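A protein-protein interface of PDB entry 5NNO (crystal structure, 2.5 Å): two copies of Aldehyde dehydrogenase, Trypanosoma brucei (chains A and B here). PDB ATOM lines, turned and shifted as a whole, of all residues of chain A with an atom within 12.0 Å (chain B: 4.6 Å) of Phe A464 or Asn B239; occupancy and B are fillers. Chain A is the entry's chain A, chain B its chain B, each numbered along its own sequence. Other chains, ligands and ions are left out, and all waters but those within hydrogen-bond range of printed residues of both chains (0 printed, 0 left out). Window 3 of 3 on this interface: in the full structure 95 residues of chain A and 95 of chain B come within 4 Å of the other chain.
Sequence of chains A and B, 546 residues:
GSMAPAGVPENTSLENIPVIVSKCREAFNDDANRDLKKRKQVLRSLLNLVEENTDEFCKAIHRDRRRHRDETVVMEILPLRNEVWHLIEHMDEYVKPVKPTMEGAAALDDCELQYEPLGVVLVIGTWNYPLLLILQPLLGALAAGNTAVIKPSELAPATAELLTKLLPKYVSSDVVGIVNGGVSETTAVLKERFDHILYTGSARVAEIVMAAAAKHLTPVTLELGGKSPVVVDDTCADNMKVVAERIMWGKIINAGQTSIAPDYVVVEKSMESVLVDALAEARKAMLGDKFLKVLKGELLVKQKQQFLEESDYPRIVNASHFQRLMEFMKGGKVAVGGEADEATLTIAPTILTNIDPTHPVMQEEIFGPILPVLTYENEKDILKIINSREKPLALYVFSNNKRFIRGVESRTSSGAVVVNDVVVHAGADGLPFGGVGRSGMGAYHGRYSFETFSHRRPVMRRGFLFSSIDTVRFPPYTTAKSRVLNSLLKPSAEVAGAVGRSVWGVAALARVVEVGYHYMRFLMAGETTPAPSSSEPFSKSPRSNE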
ATOM      1  N   LEU A 108     -23.479   0.138  19.116  1.00  0.00           N
ATOM      2  CA  LEU A 108     -23.553   0.944  20.344  1.00  0.00           C
ATOM      3  C   LEU A 108     -23.320   2.432  20.084  1.00  0.00           C
ATOM      4  O   LEU A 108     -23.580   3.267  20.957  1.00  0.00           O
ATOM      5  CB  LEU A 108     -22.535   0.451  21.375  1.00  0.00           C
ATOM      6  CG  LEU A 108     -22.774  -0.970  21.876  1.00  0.00           C
ATOM      7  CD1 LEU A 108     -21.486  -1.499  22.510  1.00  0.00           C
ATOM      8  CD2 LEU A 108     -23.971  -1.034  22.824  1.00  0.00           C
ATOM      9  N   ASP A 109     -22.802   2.754  18.901  1.00  0.00           N
ATOM     10  CA  ASP A 109     -22.373   4.112  18.563  1.00  0.00           C
ATOM     11  C   ASP A 109     -23.501   4.819  17.796  1.00  0.00           C
ATOM     12  O   ASP A 109     -24.549   4.218  17.565  1.00  0.00           O
ATOM     13  CB  ASP A 109     -21.073   4.043  17.746  1.00  0.00           C
ATOM     14  CG  ASP A 109     -19.944   3.274  18.488  1.00  0.00           C
ATOM     15  OD1 ASP A 109     -19.820   3.430  19.732  1.00  0.00           O
ATOM     16  OD2 ASP A 109     -19.173   2.531  17.836  1.00  0.00           O
ATOM     17  N   ASP A 110     -23.295   6.094  17.450  1.00  0.00           N
ATOM     18  CA  ASP A 110     -24.240   6.866  16.624  1.00  0.00           C
ATOM     19  C   ASP A 110     -23.596   7.019  15.270  1.00  0.00           C
ATOM     20  O   ASP A 110     -22.576   7.670  15.150  1.00  0.00           O
ATOM     21  CB  ASP A 110     -24.527   8.254  17.232  1.00  0.00           C
ATOM     22  CG  ASP A 110     -25.212   9.223  16.240  1.00  0.00           C
ATOM     23  OD1 ASP A 110     -25.877   8.765  15.285  1.00  0.00           O
ATOM     24  OD2 ASP A 110     -25.055  10.461  16.423  1.00  0.00           O
ATOM     25  N   MET A 460     -19.128   8.476  12.077  1.00  0.00           N
ATOM     26  CA  MET A 460     -19.328   7.714  13.320  1.00  0.00           C
ATOM     27  C   MET A 460     -19.086   8.666  14.478  1.00  0.00           C
ATOM     28  O   MET A 460     -18.069   9.358  14.520  1.00  0.00           O
ATOM     29  CB  MET A 460     -18.362   6.506  13.389  1.00  0.00           C
ATOM     30  CG  MET A 460     -18.471   5.653  14.660  1.00  0.00           C
ATOM     31  SD  MET A 460     -17.274   4.302  14.915  1.00  0.00           S
ATOM     32  CE  MET A 460     -18.044   3.011  13.959  1.00  0.00           C
ATOM     33  N   ARG A 461     -20.010   8.688  15.435  1.00  0.00           N
ATOM     34  CA  ARG A 461     -19.826   9.466  16.665  1.00  0.00           C
ATOM     35  C   ARG A 461     -19.684   8.492  17.824  1.00  0.00           C
ATOM     36  O   ARG A 461     -20.513   7.612  17.989  1.00  0.00           O
ATOM     37  CB  ARG A 461     -20.976  10.472  16.876  1.00  0.00           C
ATOM     38  CG  ARG A 461     -21.258  11.345  15.637  1.00  0.00           C
ATOM     39  CD  ARG A 461     -21.885  12.703  15.935  1.00  0.00           C
ATOM     40  NE  ARG A 461     -22.107  13.460  14.692  1.00  0.00           N
ATOM     41  CZ  ARG A 461     -23.173  13.320  13.867  1.00  0.00           C
ATOM     42  NH1 ARG A 461     -24.178  12.467  14.126  1.00  0.00           N
ATOM     43  NH2 ARG A 461     -23.249  14.042  12.745  1.00  0.00           N
ATOM     44  N   ARG A 462     -18.592   8.639  18.588  1.00  0.00           N
ATOM     45  CA  ARG A 462     -18.366   7.906  19.832  1.00  0.00           C
ATOM     46  C   ARG A 462     -18.218   8.864  20.995  1.00  0.00           C
ATOM     47  O   ARG A 462     -17.938  10.051  20.804  1.00  0.00           O
ATOM     48  CB  ARG A 462     -17.090   7.079  19.760  1.00  0.00           C
ATOM     49  CG  ARG A 462     -17.033   6.133  18.580  1.00  0.00           C
ATOM     50  CD  ARG A 462     -16.013   5.027  18.748  1.00  0.00           C
ATOM     51  NE  ARG A 462     -15.848   4.601  20.152  1.00  0.00           N
ATOM     52  CZ  ARG A 462     -16.298   3.474  20.694  1.00  0.00           C
ATOM     53  NH1 ARG A 462     -16.959   2.573  19.981  1.00  0.00           N
ATOM     54  NH2 ARG A 462     -16.099   3.238  21.980  1.00  0.00           N
ATOM     55  N   GLY A 463     -18.400   8.320  22.198  1.00  0.00           N
ATOM     56  CA  GLY A 463     -18.157   9.032  23.459  1.00  0.00           C
ATOM     57  C   GLY A 463     -16.798   8.654  24.000  1.00  0.00           C
ATOM     58  O   GLY A 463     -16.083   7.859  23.390  1.00  0.00           O
ATOM     59  N   PHE A 464     -16.448   9.193  25.162  1.00  0.00           N
ATOM     60  CA  PHE A 464     -15.150   8.876  25.802  1.00  0.00           C
ATOM     61  C   PHE A 464     -15.203   7.746  26.847  1.00  0.00           C
ATOM     62  O   PHE A 464     -14.186   7.442  27.458  1.00  0.00           O
ATOM     63  CB  PHE A 464     -14.532  10.143  26.410  1.00  0.00           C
ATOM     64  CG  PHE A 464     -13.942  11.090  25.383  1.00  0.00           C
ATOM     65  CD1 PHE A 464     -12.807  10.728  24.655  1.00  0.00           C
ATOM     66  CD2 PHE A 464     -14.499  12.355  25.161  1.00  0.00           C
ATOM     67  CE1 PHE A 464     -12.251  11.599  23.730  1.00  0.00           C
ATOM     68  CE2 PHE A 464     -13.946  13.220  24.231  1.00  0.00           C
ATOM     69  CZ  PHE A 464     -12.820  12.844  23.518  1.00  0.00           C
ATOM     70  N   LEU A 465     -16.351   7.080  26.983  1.00  0.00           N
ATOM     71  CA  LEU A 465     -16.580   6.076  28.034  1.00  0.00           C
ATOM     72  C   LEU A 465     -16.174   4.665  27.552  1.00  0.00           C
ATOM     73  O   LEU A 465     -15.935   4.452  26.354  1.00  0.00           O
ATOM     74  CB  LEU A 465     -18.058   6.074  28.443  1.00  0.00           C
ATOM     75  CG  LEU A 465     -18.850   7.364  28.751  1.00  0.00           C
ATOM     76  CD1 LEU A 465     -18.703   7.802  30.208  1.00  0.00           C
ATOM     77  CD2 LEU A 465     -18.650   8.565  27.815  1.00  0.00           C
ATOM     78  N   PHE A 466     -16.079   3.720  28.491  1.00  0.00           N
ATOM     79  CA  PHE A 466     -15.639   2.341  28.192  1.00  0.00           C
ATOM     80  C   PHE A 466     -16.628   1.609  27.270  1.00  0.00           C
ATOM     81  O   PHE A 466     -17.845   1.822  27.355  1.00  0.00           O
ATOM     82  CB  PHE A 466     -15.461   1.552  29.492  1.00  0.00           C
ATOM     83  CG  PHE A 466     -14.795   0.203  29.318  1.00  0.00           C
ATOM     84  CD1 PHE A 466     -13.432   0.109  29.034  1.00  0.00           C
ATOM     85  CD2 PHE A 466     -15.526  -0.985  29.470  1.00  0.00           C
ATOM     86  CE1 PHE A 466     -12.808  -1.133  28.890  1.00  0.00           C
ATOM     87  CE2 PHE A 466     -14.902  -2.230  29.324  1.00  0.00           C
ATOM     88  CZ  PHE A 466     -13.544  -2.302  29.031  1.00  0.00           C
ATOM     89  N   SER A 467     -16.093   0.760  26.386  1.00  0.00           N
ATOM     90  CA  SER A 467     -16.904  -0.055  25.465  1.00  0.00           C
ATOM     91  C   SER A 467     -16.198  -1.375  25.109  1.00  0.00           C
ATOM     92  O   SER A 467     -14.988  -1.541  25.381  1.00  0.00           O
ATOM     93  CB  SER A 467     -17.254   0.740  24.208  1.00  0.00           C
ATOM     94  OG  SER A 467     -16.152   0.910  23.336  1.00  0.00           O
ATOM     95  N   SER A 468     -16.960  -2.299  24.511  1.00  0.00           N
ATOM     96  CA  SER A 468     -16.498  -3.682  24.230  1.00  0.00           C
ATOM     97  C   SER A 468     -15.065  -3.768  23.688  1.00  0.00           C
ATOM     98  O   SER A 468     -14.254  -4.559  24.181  1.00  0.00           O
ATOM     99  CB  SER A 468     -17.441  -4.362  23.223  1.00  0.00           C
ATOM    100  OG  SER A 468     -17.580  -3.589  22.042  1.00  0.00           O
ATOM    101  N   ILE A 469     -14.775  -2.917  22.697  1.00  0.00           N
ATOM    102  CA  ILE A 469     -13.501  -2.938  21.957  1.00  0.00           C
ATOM    103  C   ILE A 469     -12.246  -2.676  22.799  1.00  0.00           C
ATOM    104  O   ILE A 469     -11.177  -3.186  22.470  1.00  0.00           O
ATOM    105  CB  ILE A 469     -13.491  -1.936  20.755  1.00  0.00           C
ATOM    106  CG1 ILE A 469     -13.567  -0.462  21.203  1.00  0.00           C
ATOM    107  CG2 ILE A 469     -14.619  -2.218  19.770  1.00  0.00           C
ATOM    108  CD1 ILE A 469     -13.038   0.478  20.136  1.00  0.00           C
ATOM    109  N   ASP A 470     -12.371  -1.882  23.867  1.00  0.00           N
ATOM    110  CA  ASP A 470     -11.214  -1.503  24.700  1.00  0.00           C
ATOM    111  C   ASP A 470     -10.577  -2.643  25.509  1.00  0.00           C
ATOM    112  O   ASP A 470      -9.467  -2.486  26.015  1.00  0.00           O
ATOM    113  CB  ASP A 470     -11.574  -0.351  25.646  1.00  0.00           C
ATOM    114  CG  ASP A 470     -11.767   0.982  24.923  1.00  0.00           C
ATOM    115  OD1 ASP A 470     -11.083   1.237  23.910  1.00  0.00           O
ATOM    116  OD2 ASP A 470     -12.601   1.791  25.392  1.00  0.00           O
ATOM    117  N   THR A 471     -11.264  -3.776  25.637  1.00  0.00           N
ATOM    118  CA  THR A 471     -10.703  -4.972  26.295  1.00  0.00           C
ATOM    119  C   THR A 471      -9.558  -5.627  25.518  1.00  0.00           C
ATOM    120  O   THR A 471      -8.774  -6.356  26.114  1.00  0.00           O
ATOM    121  CB  THR A 471     -11.777  -6.060  26.548  1.00  0.00           C
ATOM    122  OG1 THR A 471     -12.491  -6.327  25.338  1.00  0.00           O
ATOM    123  CG2 THR A 471     -12.758  -5.617  27.596  1.00  0.00           C
ATOM    124  N   ARG A 473      -7.850  -3.940  22.289  1.00  0.00           N
ATOM    125  CA  ARG A 473      -7.103  -3.157  21.292  1.00  0.00           C
ATOM    126  C   ARG A 473      -5.712  -2.672  21.763  1.00  0.00           C
ATOM    127  O   ARG A 473      -4.726  -2.856  21.056  1.00  0.00           O
ATOM    128  CB  ARG A 473      -7.954  -2.017  20.692  1.00  0.00           C
ATOM    129  CG  ARG A 473      -8.247  -0.813  21.576  1.00  0.00           C
ATOM    130  CD  ARG A 473      -8.632   0.398  20.731  1.00  0.00           C
ATOM    131  NE  ARG A 473      -9.700   1.203  21.331  1.00  0.00           N
ATOM    132  CZ  ARG A 473     -10.137   2.374  20.861  1.00  0.00           C
ATOM    133  NH1 ARG A 473     -11.126   3.006  21.486  1.00  0.00           N
ATOM    134  NH2 ARG A 473      -9.573   2.937  19.804  1.00  0.00           N
ATOM    135  N   PHE A 474      -5.631  -2.098  22.961  1.00  0.00           N
ATOM    136  CA  PHE A 474      -4.431  -1.349  23.379  1.00  0.00           C
ATOM    137  C   PHE A 474      -3.253  -2.239  23.799  1.00  0.00           C
ATOM    138  O   PHE A 474      -3.411  -3.098  24.662  1.00  0.00           O
ATOM    139  CB  PHE A 474      -4.787  -0.379  24.503  1.00  0.00           C
ATOM    140  CG  PHE A 474      -5.808   0.658  24.102  1.00  0.00           C
ATOM    141  CD1 PHE A 474      -5.488   1.628  23.147  1.00  0.00           C
ATOM    142  CD2 PHE A 474      -7.079   0.680  24.667  1.00  0.00           C
ATOM    143  CE1 PHE A 474      -6.411   2.592  22.763  1.00  0.00           C
ATOM    144  CE2 PHE A 474      -8.001   1.644  24.289  1.00  0.00           C
ATOM    145  CZ  PHE A 474      -7.670   2.600  23.335  1.00  0.00           C
ATOM    146  N   THR B 235     -12.253  21.514  24.303  1.00  0.00           N
ATOM    147  CA  THR B 235     -13.364  21.018  25.117  1.00  0.00           C
ATOM    148  C   THR B 235     -13.102  19.581  25.619  1.00  0.00           C
ATOM    149  O   THR B 235     -14.014  18.946  26.171  1.00  0.00           O
ATOM    150  CB  THR B 235     -14.710  21.094  24.336  1.00  0.00           C
ATOM    151  OG1 THR B 235     -14.636  20.308  23.133  1.00  0.00           O
ATOM    152  CG2 THR B 235     -15.038  22.521  23.971  1.00  0.00           C
ATOM    153  N   CYS B 236     -11.869  19.085  25.433  1.00  0.00           N
ATOM    154  CA  CYS B 236     -11.480  17.714  25.822  1.00  0.00           C
ATOM    155  C   CYS B 236     -10.496  17.618  26.971  1.00  0.00           C
ATOM    156  O   CYS B 236      -9.925  16.560  27.159  1.00  0.00           O
ATOM    157  CB  CYS B 236     -10.813  16.999  24.640  1.00  0.00           C
ATOM    158  SG  CYS B 236     -11.745  17.063  23.111  1.00  0.00           S
ATOM    159  N   ALA B 237     -10.301  18.694  27.735  1.00  0.00           N
ATOM    160  CA  ALA B 237      -9.238  18.747  28.749  1.00  0.00           C
ATOM    161  C   ALA B 237      -9.325  17.594  29.732  1.00  0.00           C
ATOM    162  O   ALA B 237      -8.334  16.904  29.977  1.00  0.00           O
ATOM    163  CB  ALA B 237      -9.272  20.059  29.495  1.00  0.00           C
ATOM    164  N   ASP B 238     -10.515  17.367  30.261  1.00  0.00           N
ATOM    165  CA  ASP B 238     -10.760  16.305  31.252  1.00  0.00           C
ATOM    166  C   ASP B 238     -10.596  14.862  30.696  1.00  0.00           C
ATOM    167  O   ASP B 238     -10.346  13.940  31.454  1.00  0.00           O
ATOM    168  CB  ASP B 238     -12.168  16.483  31.870  1.00  0.00           C
ATOM    169  CG  ASP B 238     -12.380  17.862  32.506  1.00  0.00           C
ATOM    170  OD1 ASP B 238     -11.412  18.444  33.054  1.00  0.00           O
ATOM    171  OD2 ASP B 238     -13.531  18.358  32.477  1.00  0.00           O
ATOM    172  N   ASN B 239     -10.749  14.695  29.380  1.00  0.00           N
ATOM    173  CA  ASN B 239     -10.685  13.397  28.684  1.00  0.00           C
ATOM    174  C   ASN B 239      -9.337  13.184  27.968  1.00  0.00           C
ATOM    175  O   ASN B 239      -9.188  12.196  27.227  1.00  0.00           O
ATOM    176  CB  ASN B 239     -11.798  13.292  27.603  1.00  0.00           C
ATOM    177  CG  ASN B 239     -13.142  13.861  28.063  1.00  0.00           C
ATOM    178  OD1 ASN B 239     -13.786  13.314  28.951  1.00  0.00           O
ATOM    179  ND2 ASN B 239     -13.571  14.956  27.447  1.00  0.00           N
ATOM    180  N   MET B 240      -8.360  14.089  28.176  1.00  0.00           N
ATOM    181  CA  MET B 240      -7.095  14.086  27.390  1.00  0.00           C
ATOM    182  C   MET B 240      -6.344  12.742  27.352  1.00  0.00           C
ATOM    183  O   MET B 240      -5.670  12.434  26.359  1.00  0.00           O
ATOM    184  CB  MET B 240      -6.140  15.193  27.863  1.00  0.00           C
ATOM    185  CG  MET B 240      -4.949  15.466  26.955  1.00  0.00           C
ATOM    186  SD  MET B 240      -5.391  15.921  25.272  1.00  0.00           S
ATOM    187  CE  MET B 240      -6.134  17.537  25.532  1.00  0.00           C
ATOM    188  N   LYS B 241      -6.460  11.953  28.418  1.00  0.00           N
ATOM    189  CA  LYS B 241      -5.856  10.609  28.457  1.00  0.00           C
ATOM    190  C   LYS B 241      -6.515   9.612  27.468  1.00  0.00           C
ATOM    191  O   LYS B 241      -5.837   8.761  26.905  1.00  0.00           O
ATOM    192  CB  LYS B 241      -5.869  10.074  29.895  1.00  0.00           C
ATOM    193  CG  LYS B 241      -5.168   8.736  30.095  1.00  0.00           C
ATOM    194  CD  LYS B 241      -4.455   8.666  31.461  1.00  0.00           C
ATOM    195  CE  LYS B 241      -4.316   7.260  32.053  1.00  0.00           C
ATOM    196  NZ  LYS B 241      -4.014   6.180  31.088  1.00  0.00           N
ATOM    197  N   VAL B 242      -7.817   9.743  27.241  1.00  0.00           N
ATOM    198  CA  VAL B 242      -8.524   8.897  26.262  1.00  0.00           C
ATOM    199  C   VAL B 242      -8.197   9.333  24.824  1.00  0.00           C
ATOM    200  O   VAL B 242      -7.981   8.479  23.943  1.00  0.00           O
ATOM    201  CB  VAL B 242     -10.061   8.893  26.448  1.00  0.00           C
ATOM    202  CG1 VAL B 242     -10.707   7.923  25.447  1.00  0.00           C
ATOM    203  CG2 VAL B 242     -10.456   8.471  27.851  1.00  0.00           C
ATOM    204  N   VAL B 243      -8.167  10.651  24.622  1.00  0.00           N
ATOM    205  CA  VAL B 243      -7.797  11.296  23.346  1.00  0.00           C
ATOM    206  C   VAL B 243      -6.394  10.893  22.917  1.00  0.00           C
ATOM    207  O   VAL B 243      -6.142  10.576  21.751  1.00  0.00           O
ATOM    208  CB  VAL B 243      -7.843  12.856  23.443  1.00  0.00           C
ATOM    209  CG1 VAL B 243      -7.329  13.524  22.175  1.00  0.00           C
ATOM    210  CG2 VAL B 243      -9.244  13.363  23.749  1.00  0.00           C
ATOM    211  N   ARG B 246      -6.042   6.919  22.260  1.00  0.00           N
ATOM    212  CA  ARG B 246      -6.684   6.548  20.977  1.00  0.00           C
ATOM    213  C   ARG B 246      -5.864   6.979  19.775  1.00  0.00           C
ATOM    214  O   ARG B 246      -5.702   6.197  18.838  1.00  0.00           O
ATOM    215  CB  ARG B 246      -8.114   7.080  20.900  1.00  0.00           C
ATOM    216  CG  ARG B 246      -9.034   6.270  21.774  1.00  0.00           C
ATOM    217  CD  ARG B 246     -10.377   6.924  21.958  1.00  0.00           C
ATOM    218  NE  ARG B 246     -11.216   6.131  22.865  1.00  0.00           N
ATOM    219  CZ  ARG B 246     -12.470   6.422  23.199  1.00  0.00           C
ATOM    220  NH1 ARG B 246     -13.080   7.486  22.693  1.00  0.00           N
ATOM    221  NH2 ARG B 246     -13.117   5.638  24.049  1.00  0.00           N
ATOM    222  N   PHE B 398     -11.675  15.283  17.704  1.00  0.00           N
ATOM    223  CA  PHE B 398     -11.826  15.089  19.146  1.00  0.00           C
ATOM    224  C   PHE B 398     -12.475  16.328  19.748  1.00  0.00           C
ATOM    225  O   PHE B 398     -11.931  17.417  19.675  1.00  0.00           O
ATOM    226  CB  PHE B 398     -10.480  14.746  19.771  1.00  0.00           C
ATOM    227  CG  PHE B 398     -10.037  13.339  19.462  1.00  0.00           C
ATOM    228  CD1 PHE B 398      -9.442  13.042  18.251  1.00  0.00           C
ATOM    229  CD2 PHE B 398     -10.270  12.309  20.363  1.00  0.00           C
ATOM    230  CE1 PHE B 398      -9.045  11.752  17.960  1.00  0.00           C
ATOM    231  CE2 PHE B 398      -9.889  11.009  20.069  1.00  0.00           C
ATOM    232  CZ  PHE B 398      -9.273  10.729  18.862  1.00  0.00           C
ATOM    233  N   ASN B 400     -16.209  17.655  22.405  1.00  0.00           N
ATOM    234  CA  ASN B 400     -17.466  17.543  23.135  1.00  0.00           C
ATOM    235  C   ASN B 400     -18.431  18.680  22.743  1.00  0.00           C
ATOM    236  O   ASN B 400     -19.534  18.755  23.305  1.00  0.00           O
ATOM    237  CB  ASN B 400     -17.199  17.636  24.654  1.00  0.00           C
ATOM    238  CG  ASN B 400     -16.583  16.373  25.235  1.00  0.00           C
ATOM    239  OD1 ASN B 400     -15.419  16.341  25.625  1.00  0.00           O
ATOM    240  ND2 ASN B 400     -17.384  15.338  25.323  1.00  0.00           N
ATOM    241  N   ASN B 420     -14.249  11.451  18.173  1.00  0.00           N
ATOM    242  CA  ASN B 420     -13.725  10.943  19.469  1.00  0.00           C
ATOM    243  C   ASN B 420     -12.978   9.577  19.440  1.00  0.00           C
ATOM    244  O   ASN B 420     -12.746   8.970  20.483  1.00  0.00           O
ATOM    245  CB  ASN B 420     -14.801  10.965  20.569  1.00  0.00           C
ATOM    246  CG  ASN B 420     -15.276  12.377  20.921  1.00  0.00           C
ATOM    247  OD1 ASN B 420     -14.581  13.355  20.703  1.00  0.00           O
ATOM    248  ND2 ASN B 420     -16.454  12.478  21.505  1.00  0.00           N
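No position is printed for both chains.
Of the 11 pairs that touch across the chains among the printed residues, none has its exchanged pair printed and touching as well.
The guanidinium group (NH1) of Arg B246 is in hydrogen-bond range of the backbone carbonyl oxygen (O) of Asn B420 (2.7 Å).
ND2 of Asn B239 lies within hydrogen-bond range of OD1 of Asn B400 (2.9 Å).
NE of Arg A473 lies within salt-bridge range of OD1 of Asp A470, 2.9 Å away.
OG of Ser A467 lies within hydrogen-bond range of NH2 of Arg A462 (2.7 Å).
The side-chain carboxylate (OD1) of Asp A109 lies within salt-bridge range of the guanidinium group (NH1) of Arg A462.
O of Phe B398 sits at hydrogen-bond distance from SG of Cys B236 (3.5 Å).
Among the printed residues, merely in contact across the chains: Phe A464 with Asn B420, Phe A464 with Val B243, Phe A464 with Asn B239, Phe A464 with Val B242, Phe A464 with Asn B400, Phe A464 with Arg B246, Leu A465 with Arg B246 and Phe A464 with Phe B398.
Of the 17 printed residues of chain A, 5 touch a printed residue of chain B.
Of the 13 printed residues of chain B, 7 touch a printed residue of chain A.
Phe A464 touches seven residues of chain B.
Of the printed residues of chain A, Asn B239 touches Phe A464 (3.5 Å).
No residue of chain A comes within 4 Å of Met B240.
Of chain A, only Phe A464 comes within 4 Å of Val B243.
Phe B398 touches just one residue of chain A: Phe A464 (3.97 Å).
Of chain A, only Phe A464 comes within 4 Å of Asn B400.
Asn B420 touches just these residues of chain A: Arg A462 and Phe A464.
Of the printed residues of chain A, Arg B246 touches Gly A463 (3.1 Å), Phe A464 (3.8 Å), Leu A465 (3.8 Å) and Arg A473 (3.4 Å).
Printed residues of chain B within 4 Å of Arg A473: Arg B246.
Asp A110 touches none of the printed residues of chain B.
Met A460 touches none of the printed residues of chain B.
The nearest residue of chain B that does not touch Phe A464 is Cys B236 (4.4 Å).
The nearest residue of chain A that does not touch Asn B239 is Leu A465 (6.9 Å).
The nearest printed residue of chain B that does not touch Arg A462 is Arg B246 (4.4 Å).
NH1 of Arg A473 lies close to NE of Arg B246 (3.4 Å).
NH1 of Arg B246 is in hydrogen-bond range of O of Gly A463 (3.1 Å).
ND2 of Asn B420 is in hydrogen-bond range of O of Arg A462, at 2.9 Å.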
